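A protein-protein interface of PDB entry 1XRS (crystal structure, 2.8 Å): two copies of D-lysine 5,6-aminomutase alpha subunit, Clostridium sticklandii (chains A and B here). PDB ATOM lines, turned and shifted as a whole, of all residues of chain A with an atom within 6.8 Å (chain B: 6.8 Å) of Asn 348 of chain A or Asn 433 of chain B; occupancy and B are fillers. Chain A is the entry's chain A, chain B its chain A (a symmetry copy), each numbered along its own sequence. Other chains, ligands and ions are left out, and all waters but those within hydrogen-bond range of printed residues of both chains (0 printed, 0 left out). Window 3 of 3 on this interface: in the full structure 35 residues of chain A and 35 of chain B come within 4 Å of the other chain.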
ATOM      1  N   MET A 342      37.882   1.645 -23.641  1.00  0.00           N
ATOM      2  CA  MET A 342      37.423   2.917 -24.203  1.00  0.00           C
ATOM      3  C   MET A 342      36.680   3.722 -23.144  1.00  0.00           C
ATOM      4  O   MET A 342      36.106   3.194 -22.192  1.00  0.00           O
ATOM      5  CB  MET A 342      36.514   2.724 -25.398  1.00  0.00           C
ATOM      6  CG  MET A 342      37.218   2.293 -26.650  1.00  0.00           C
ATOM      7  SD  MET A 342      35.965   1.948 -27.892  1.00  0.00           S
ATOM      8  CE  MET A 342      36.778   0.749 -28.942  1.00  0.00           C
ATOM      9  N   PRO A 344      34.123   5.505 -20.998  1.00  0.00           N
ATOM     10  CA  PRO A 344      32.701   5.214 -20.784  1.00  0.00           C
ATOM     11  C   PRO A 344      31.718   6.310 -21.293  1.00  0.00           C
ATOM     12  O   PRO A 344      30.547   6.034 -21.542  1.00  0.00           O
ATOM     13  CB  PRO A 344      32.627   4.962 -19.270  1.00  0.00           C
ATOM     14  CG  PRO A 344      33.741   5.800 -18.706  1.00  0.00           C
ATOM     15  CD  PRO A 344      34.852   5.619 -19.722  1.00  0.00           C
ATOM     16  N   GLU A 345      32.199   7.537 -21.478  1.00  0.00           N
ATOM     17  CA  GLU A 345      31.352   8.639 -21.984  1.00  0.00           C
ATOM     18  C   GLU A 345      31.301   8.712 -23.516  1.00  0.00           C
ATOM     19  O   GLU A 345      30.696   9.620 -24.086  1.00  0.00           O
ATOM     20  CB  GLU A 345      31.831  10.004 -21.427  1.00  0.00           C
ATOM     21  CG  GLU A 345      31.231  10.407 -20.076  1.00  0.00           C
ATOM     22  CD  GLU A 345      30.795   9.183 -19.240  1.00  0.00           C
ATOM     23  OE1 GLU A 345      31.663   8.342 -18.911  1.00  0.00           O
ATOM     24  OE2 GLU A 345      29.583   9.047 -18.926  1.00  0.00           O
ATOM     25  N   LEU A 346      31.946   7.766 -24.184  1.00  0.00           N
ATOM     26  CA  LEU A 346      31.969   7.739 -25.641  1.00  0.00           C
ATOM     27  C   LEU A 346      30.625   7.255 -26.213  1.00  0.00           C
ATOM     28  O   LEU A 346      30.131   6.161 -25.865  1.00  0.00           O
ATOM     29  CB  LEU A 346      33.125   6.833 -26.118  1.00  0.00           C
ATOM     30  CG  LEU A 346      33.210   6.442 -27.604  1.00  0.00           C
ATOM     31  CD1 LEU A 346      33.173   7.706 -28.449  1.00  0.00           C
ATOM     32  CD2 LEU A 346      34.464   5.606 -27.897  1.00  0.00           C
ATOM     33  N   LYS A 347      30.015   8.063 -27.079  1.00  0.00           N
ATOM     34  CA  LYS A 347      28.740   7.639 -27.646  1.00  0.00           C
ATOM     35  C   LYS A 347      28.935   6.336 -28.433  1.00  0.00           C
ATOM     36  O   LYS A 347      29.915   6.174 -29.160  1.00  0.00           O
ATOM     37  CB  LYS A 347      28.122   8.732 -28.547  1.00  0.00           C
ATOM     38  CG  LYS A 347      26.870   8.237 -29.270  1.00  0.00           C
ATOM     39  CD  LYS A 347      26.293   9.258 -30.232  1.00  0.00           C
ATOM     40  CE  LYS A 347      25.666  10.430 -29.505  1.00  0.00           C
ATOM     41  NZ  LYS A 347      24.950  11.289 -30.484  1.00  0.00           N
ATOM     42  N   ASN A 348      27.991   5.419 -28.272  1.00  0.00           N
ATOM     43  CA  ASN A 348      28.038   4.136 -28.930  1.00  0.00           C
ATOM     44  C   ASN A 348      29.310   3.388 -28.574  1.00  0.00           C
ATOM     45  O   ASN A 348      29.594   2.344 -29.161  1.00  0.00           O
ATOM     46  CB  ASN A 348      27.933   4.287 -30.457  1.00  0.00           C
ATOM     47  CG  ASN A 348      26.480   4.418 -30.948  1.00  0.00           C
ATOM     48  OD1 ASN A 348      25.630   3.559 -30.684  1.00  0.00           O
ATOM     49  ND2 ASN A 348      26.193   5.503 -31.653  1.00  0.00           N
ATOM     50  N   GLY A 349      30.087   3.921 -27.633  1.00  0.00           N
ATOM     51  CA  GLY A 349      31.297   3.246 -27.235  1.00  0.00           C
ATOM     52  C   GLY A 349      31.124   1.727 -27.035  1.00  0.00           C
ATOM     53  O   GLY A 349      31.890   0.932 -27.582  1.00  0.00           O
ATOM     54  N   PHE A 350      30.137   1.307 -26.246  1.00  0.00           N
ATOM     55  CA  PHE A 350      29.915  -0.119 -26.013  1.00  0.00           C
ATOM     56  C   PHE A 350      29.738  -0.909 -27.334  1.00  0.00           C
ATOM     57  O   PHE A 350      30.109  -2.089 -27.421  1.00  0.00           O
ATOM     58  CB  PHE A 350      28.689  -0.305 -25.098  1.00  0.00           C
ATOM     59  CG  PHE A 350      28.237  -1.726 -24.966  1.00  0.00           C
ATOM     60  CD1 PHE A 350      27.195  -2.205 -25.732  1.00  0.00           C
ATOM     61  CD2 PHE A 350      28.880  -2.602 -24.081  1.00  0.00           C
ATOM     62  CE1 PHE A 350      26.796  -3.565 -25.617  1.00  0.00           C
ATOM     63  CE2 PHE A 350      28.494  -3.954 -23.955  1.00  0.00           C
ATOM     64  CZ  PHE A 350      27.454  -4.430 -24.725  1.00  0.00           C
ATOM     65  N   LEU A 351      29.169  -0.265 -28.351  1.00  0.00           N
ATOM     66  CA  LEU A 351      29.013  -0.911 -29.646  1.00  0.00           C
ATOM     67  C   LEU A 351      30.401  -1.085 -30.294  1.00  0.00           C
ATOM     68  O   LEU A 351      30.677  -2.119 -30.887  1.00  0.00           O
ATOM     69  CB  LEU A 351      28.076  -0.106 -30.555  1.00  0.00           C
ATOM     70  CG  LEU A 351      26.604  -0.104 -30.133  1.00  0.00           C
ATOM     71  CD1 LEU A 351      25.809   0.632 -31.184  1.00  0.00           C
ATOM     72  CD2 LEU A 351      26.047  -1.555 -29.990  1.00  0.00           C
ATOM     73  N   TYR A 352      31.288  -0.103 -30.178  1.00  0.00           N
ATOM     74  CA  TYR A 352      32.616  -0.280 -30.755  1.00  0.00           C
ATOM     75  C   TYR A 352      33.429  -1.384 -30.035  1.00  0.00           C
ATOM     76  O   TYR A 352      34.182  -2.135 -30.675  1.00  0.00           O
ATOM     77  CB  TYR A 352      33.396   1.035 -30.729  1.00  0.00           C
ATOM     78  CG  TYR A 352      32.780   2.077 -31.612  1.00  0.00           C
ATOM     79  CD1 TYR A 352      32.375   3.313 -31.095  1.00  0.00           C
ATOM     80  CD2 TYR A 352      32.530   1.805 -32.955  1.00  0.00           C
ATOM     81  CE1 TYR A 352      31.729   4.243 -31.882  1.00  0.00           C
ATOM     82  CE2 TYR A 352      31.892   2.724 -33.761  1.00  0.00           C
ATOM     83  CZ  TYR A 352      31.488   3.944 -33.223  1.00  0.00           C
ATOM     84  OH  TYR A 352      30.829   4.853 -34.042  1.00  0.00           O
ATOM     85  N   GLU A 353      33.267  -1.501 -28.722  1.00  0.00           N
ATOM     86  CA  GLU A 353      34.008  -2.492 -27.957  1.00  0.00           C
ATOM     87  C   GLU A 353      33.598  -3.882 -28.321  1.00  0.00           C
ATOM     88  O   GLU A 353      34.412  -4.747 -28.563  1.00  0.00           O
ATOM     89  CB  GLU A 353      33.766  -2.268 -26.481  1.00  0.00           C
ATOM     90  CG  GLU A 353      34.320  -0.932 -26.014  1.00  0.00           C
ATOM     91  CD  GLU A 353      35.727  -1.022 -25.500  1.00  0.00           C
ATOM     92  OE1 GLU A 353      36.097  -0.158 -24.674  1.00  0.00           O
ATOM     93  OE2 GLU A 353      36.451  -1.951 -25.911  1.00  0.00           O
ATOM     94  N   LEU A 449      27.455   0.389 -37.959  1.00  0.00           N
ATOM     95  CA  LEU A 449      28.592   0.720 -37.113  1.00  0.00           C
ATOM     96  C   LEU A 449      29.407  -0.483 -36.693  1.00  0.00           C
ATOM     97  O   LEU A 449      30.623  -0.527 -36.868  1.00  0.00           O
ATOM     98  CB  LEU A 449      28.145   1.348 -35.800  1.00  0.00           C
ATOM     99  CG  LEU A 449      27.173   2.493 -35.576  1.00  0.00           C
ATOM    100  CD1 LEU A 449      27.566   3.139 -34.240  1.00  0.00           C
ATOM    101  CD2 LEU A 449      27.217   3.518 -36.711  1.00  0.00           C
ATOM    102  N   ILE B 397      16.844   1.063 -23.975  1.00  0.00           N
ATOM    103  CA  ILE B 397      17.528   1.565 -25.161  1.00  0.00           C
ATOM    104  C   ILE B 397      17.550   0.527 -26.309  1.00  0.00           C
ATOM    105  O   ILE B 397      17.581   0.919 -27.472  1.00  0.00           O
ATOM    106  CB  ILE B 397      18.993   2.029 -24.829  1.00  0.00           C
ATOM    107  CG1 ILE B 397      19.509   2.940 -25.932  1.00  0.00           C
ATOM    108  CG2 ILE B 397      19.932   0.828 -24.660  1.00  0.00           C
ATOM    109  CD1 ILE B 397      18.967   4.337 -25.857  1.00  0.00           C
ATOM    110  N   ALA B 428      21.638   5.189 -15.823  1.00  0.00           N
ATOM    111  CA  ALA B 428      20.816   5.247 -16.997  1.00  0.00           C
ATOM    112  C   ALA B 428      21.422   6.068 -18.141  1.00  0.00           C
ATOM    113  O   ALA B 428      21.237   5.703 -19.302  1.00  0.00           O
ATOM    114  CB  ALA B 428      19.475   5.795 -16.632  1.00  0.00           C
ATOM    115  N   GLN B 429      22.139   7.159 -17.838  1.00  0.00           N
ATOM    116  CA  GLN B 429      22.712   8.014 -18.897  1.00  0.00           C
ATOM    117  C   GLN B 429      23.947   7.332 -19.477  1.00  0.00           C
ATOM    118  O   GLN B 429      24.217   7.451 -20.692  1.00  0.00           O
ATOM    119  CB  GLN B 429      23.109   9.409 -18.375  1.00  0.00           C
ATOM    120  CG  GLN B 429      22.103  10.097 -17.465  1.00  0.00           C
ATOM    121  CD  GLN B 429      21.179  11.059 -18.186  1.00  0.00           C
ATOM    122  OE1 GLN B 429      20.421  10.679 -19.091  1.00  0.00           O
ATOM    123  NE2 GLN B 429      21.232  12.317 -17.788  1.00  0.00           N
ATOM    124  N   TYR B 430      24.707   6.640 -18.616  1.00  0.00           N
ATOM    125  CA  TYR B 430      25.862   5.894 -19.094  1.00  0.00           C
ATOM    126  C   TYR B 430      25.281   4.889 -20.118  1.00  0.00           C
ATOM    127  O   TYR B 430      25.505   5.011 -21.334  1.00  0.00           O
ATOM    128  CB  TYR B 430      26.548   5.186 -17.931  1.00  0.00           C
ATOM    129  CG  TYR B 430      27.701   4.303 -18.295  1.00  0.00           C
ATOM    130  CD1 TYR B 430      28.442   4.515 -19.471  1.00  0.00           C
ATOM    131  CD2 TYR B 430      28.013   3.194 -17.519  1.00  0.00           C
ATOM    132  CE1 TYR B 430      29.461   3.632 -19.872  1.00  0.00           C
ATOM    133  CE2 TYR B 430      29.033   2.296 -17.912  1.00  0.00           C
ATOM    134  CZ  TYR B 430      29.746   2.520 -19.083  1.00  0.00           C
ATOM    135  OH  TYR B 430      30.723   1.620 -19.457  1.00  0.00           O
ATOM    136  N   ILE B 431      24.495   3.924 -19.665  1.00  0.00           N
ATOM    137  CA  ILE B 431      23.927   2.989 -20.624  1.00  0.00           C
ATOM    138  C   ILE B 431      23.220   3.632 -21.831  1.00  0.00           C
ATOM    139  O   ILE B 431      23.468   3.216 -22.970  1.00  0.00           O
ATOM    140  CB  ILE B 431      22.930   2.024 -19.975  1.00  0.00           C
ATOM    141  CG1 ILE B 431      23.616   1.231 -18.849  1.00  0.00           C
ATOM    142  CG2 ILE B 431      22.369   1.083 -21.036  1.00  0.00           C
ATOM    143  CD1 ILE B 431      24.894   0.678 -19.225  1.00  0.00           C
ATOM    144  N   PHE B 432      22.354   4.625 -21.623  1.00  0.00           N
ATOM    145  CA  PHE B 432      21.684   5.198 -22.786  1.00  0.00           C
ATOM    146  C   PHE B 432      22.636   5.791 -23.776  1.00  0.00           C
ATOM    147  O   PHE B 432      22.413   5.680 -24.968  1.00  0.00           O
ATOM    148  CB  PHE B 432      20.675   6.259 -22.401  1.00  0.00           C
ATOM    149  CG  PHE B 432      19.525   5.724 -21.620  1.00  0.00           C
ATOM    150  CD1 PHE B 432      18.636   6.586 -20.984  1.00  0.00           C
ATOM    151  CD2 PHE B 432      19.341   4.332 -21.488  1.00  0.00           C
ATOM    152  CE1 PHE B 432      17.591   6.070 -20.228  1.00  0.00           C
ATOM    153  CE2 PHE B 432      18.297   3.824 -20.726  1.00  0.00           C
ATOM    154  CZ  PHE B 432      17.424   4.690 -20.097  1.00  0.00           C
ATOM    155  N   ASN B 433      23.704   6.417 -23.301  1.00  0.00           N
ATOM    156  CA  ASN B 433      24.648   7.016 -24.223  1.00  0.00           C
ATOM    157  C   ASN B 433      25.654   6.026 -24.815  1.00  0.00           C
ATOM    158  O   ASN B 433      26.013   6.095 -25.997  1.00  0.00           O
ATOM    159  CB  ASN B 433      25.419   8.132 -23.530  1.00  0.00           C
ATOM    160  CG  ASN B 433      26.455   8.759 -24.447  1.00  0.00           C
ATOM    161  OD1 ASN B 433      26.114   9.311 -25.495  1.00  0.00           O
ATOM    162  ND2 ASN B 433      27.726   8.654 -24.078  1.00  0.00           N
ATOM    163  N   ASN B 434      26.122   5.107 -23.982  1.00  0.00           N
ATOM    164  CA  ASN B 434      27.110   4.159 -24.435  1.00  0.00           C
ATOM    165  C   ASN B 434      26.602   3.160 -25.452  1.00  0.00           C
ATOM    166  O   ASN B 434      27.389   2.653 -26.266  1.00  0.00           O
ATOM    167  CB  ASN B 434      27.690   3.394 -23.263  1.00  0.00           C
ATOM    168  CG  ASN B 434      29.140   3.085 -23.464  1.00  0.00           C
ATOM    169  OD1 ASN B 434      29.613   1.992 -23.137  1.00  0.00           O
ATOM    170  ND2 ASN B 434      29.873   4.062 -24.006  1.00  0.00           N
ATOM    171  N   MET B 435      25.297   2.882 -25.383  1.00  0.00           N
ATOM    172  CA  MET B 435      24.635   1.931 -26.272  1.00  0.00           C
ATOM    173  C   MET B 435      23.611   2.616 -27.180  1.00  0.00           C
ATOM    174  O   MET B 435      22.724   1.946 -27.712  1.00  0.00           O
ATOM    175  CB  MET B 435      23.919   0.836 -25.438  1.00  0.00           C
ATOM    176  CG  MET B 435      24.802   0.129 -24.431  1.00  0.00           C
ATOM    177  SD  MET B 435      24.134  -1.397 -23.745  1.00  0.00           S
ATOM    178  CE  MET B 435      22.608  -1.170 -24.236  1.00  0.00           C
ATOM    179  N   GLU B 436      23.742   3.927 -27.369  1.00  0.00           N
ATOM    180  CA  GLU B 436      22.764   4.714 -28.142  1.00  0.00           C
ATOM    181  C   GLU B 436      22.112   4.096 -29.360  1.00  0.00           C
ATOM    182  O   GLU B 436      20.895   4.074 -29.427  1.00  0.00           O
ATOM    183  CB  GLU B 436      23.326   6.084 -28.531  1.00  0.00           C
ATOM    184  CG  GLU B 436      22.327   6.939 -29.339  1.00  0.00           C
ATOM    185  CD  GLU B 436      22.564   8.458 -29.225  1.00  0.00           C
ATOM    186  OE1 GLU B 436      22.275   9.168 -30.211  1.00  0.00           O
ATOM    187  OE2 GLU B 436      23.020   8.952 -28.163  1.00  0.00           O
ATOM    188  N   SER B 437      22.898   3.581 -30.307  1.00  0.00           N
ATOM    189  CA  SER B 437      22.320   2.980 -31.500  1.00  0.00           C
ATOM    190  C   SER B 437      22.118   1.477 -31.412  1.00  0.00           C
ATOM    191  O   SER B 437      21.671   0.847 -32.370  1.00  0.00           O
ATOM    192  CB  SER B 437      23.171   3.291 -32.733  1.00  0.00           C
ATOM    193  OG  SER B 437      23.432   4.684 -32.810  1.00  0.00           O
ATOM    194  N   ILE B 438      22.396   0.887 -30.265  1.00  0.00           N
ATOM    195  CA  ILE B 438      22.252  -0.553 -30.152  1.00  0.00           C
ATOM    196  C   ILE B 438      20.978  -1.205 -30.702  1.00  0.00           C
ATOM    197  O   ILE B 438      21.005  -2.367 -31.045  1.00  0.00           O
ATOM    198  CB  ILE B 438      22.481  -1.038 -28.688  1.00  0.00           C
ATOM    199  CG1 ILE B 438      22.772  -2.538 -28.713  1.00  0.00           C
ATOM    200  CG2 ILE B 438      21.275  -0.726 -27.778  1.00  0.00           C
ATOM    201  CD1 ILE B 438      23.377  -3.074 -27.397  1.00  0.00           C
ATOM    202  N   GLU B 441      21.578  -1.521 -34.528  1.00  0.00           N
ATOM    203  CA  GLU B 441      22.652  -2.459 -34.756  1.00  0.00           C
ATOM    204  C   GLU B 441      22.278  -3.901 -34.519  1.00  0.00           C
ATOM    205  O   GLU B 441      22.647  -4.798 -35.309  1.00  0.00           O
ATOM    206  CB  GLU B 441      23.846  -2.089 -33.892  1.00  0.00           C
ATOM    207  CG  GLU B 441      24.547  -0.848 -34.389  1.00  0.00           C
ATOM    208  CD  GLU B 441      25.079  -0.994 -35.820  1.00  0.00           C
ATOM    209  OE1 GLU B 441      24.514  -0.335 -36.723  1.00  0.00           O
ATOM    210  OE2 GLU B 441      26.055  -1.763 -36.034  1.00  0.00           O
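The backbone carbonyl oxygen (O) of Pro 344 of chain A sits at hydrogen-bond distance from the side-chain amide nitrogen (ND2) of Asn 434 of chain B (3.2 Å).
The backbone carbonyl oxygen of Glu 345 of chain A is in hydrogen-bond range of the side-chain amide nitrogen of Asn 433 of chain B (3.1 Å).
ND2 of Asn 434 of chain B lies within hydrogen-bond range of O of Leu 346 of chain A, at 2.8 Å.
NZ of Lys 347 of chain A lies within salt-bridge range of OE1 of Glu 436 of chain B.
N of Asn 348 of chain A sits at hydrogen-bond distance from O of Asn 433 of chain B (3.1 Å).
The backbone carbonyl oxygen of Asn 434 of chain B sits close to the backbone NH of Asn 348 of chain A (3.5 Å).
The side-chain amide oxygen (OD1) of Asn 348 of chain A lies within hydrogen-bond range of the backbone NH (N) of Ser 437 of chain B, at 2.8 Å.
O of Asn 434 of chain B lies within hydrogen-bond range of N of Gly 349 of chain A (3.3 Å).
The backbone NH (N) of Phe 350 of chain A sits at hydrogen-bond distance from the backbone carbonyl oxygen (O) of Asn 434 of chain B (3.1 Å).
The backbone NH (N) of Leu 449 of chain A lies within hydrogen-bond range of the side-chain carboxylate (OE2) of Glu 441 of chain B, at 3.2 Å.
Among the printed residues, pairs that only touch across the chains: Pro 344 of chain A with Tyr 430 of chain B (3.1 Å), Lys 347 of chain A with Asn 433 of chain B (3.5 Å), Leu 351 of chain A with Ile 438 of chain B (3.5 Å), Phe 350 of chain A with Met 435 of chain B (3.6 Å), Leu 351 of chain A with Glu 441 of chain B (3.7 Å), Leu 351 of chain A with Ser 437 of chain B (3.8 Å), Asn 348 of chain A with Glu 436 of chain B (3.8 Å), Leu 346 of chain A with Asn 433 of chain B (3.9 Å) and Phe 350 of chain A with Ile 438 of chain B (3.9 Å).
Met 342 of chain A touches none of the printed residues of chain B.
Of the printed residues of chain B, Glu 345 of chain A touches Asn 433 (3.1 Å).
Printed residues of chain B within 4 Å of Leu 346 of chain A: Asn 433 and Asn 434.
Of chain B, only Asn 433 (3.1 Å), Asn 434 (3.1 Å), Glu 436 (3.8 Å) and Ser 437 (2.8 Å) come within 4 Å of Asn 348 of chain A.
Printed residues of chain B within 4 Å of Leu 449 of chain A: Glu 441.
Ala 428 of chain B touches none of the printed residues of chain A.
Asn 433 of chain B touches just these residues of chain A: Glu 345, Leu 346, Lys 347 and Asn 348.
Printed residues of chain A within 4 Å of Ser 437 of chain B: Asn 348 and Leu 351.
The nearest residue of chain A that does not touch Asn 433 of chain B is Pro 344 of chain A (4.6 Å).
Of the 12 printed residues of chain A, 9 touch a printed residue of chain B.
Of the 13 printed residues of chain B, 8 touch a printed residue of chain A.
Among the printed residues, Asp or Glu carboxylates within 4 Å of a Lys or Arg side-chain nitrogen of the other chain: Lys 347 of chain A with Glu 436 of chain B (3.4 Å).
No position is printed for both chains.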
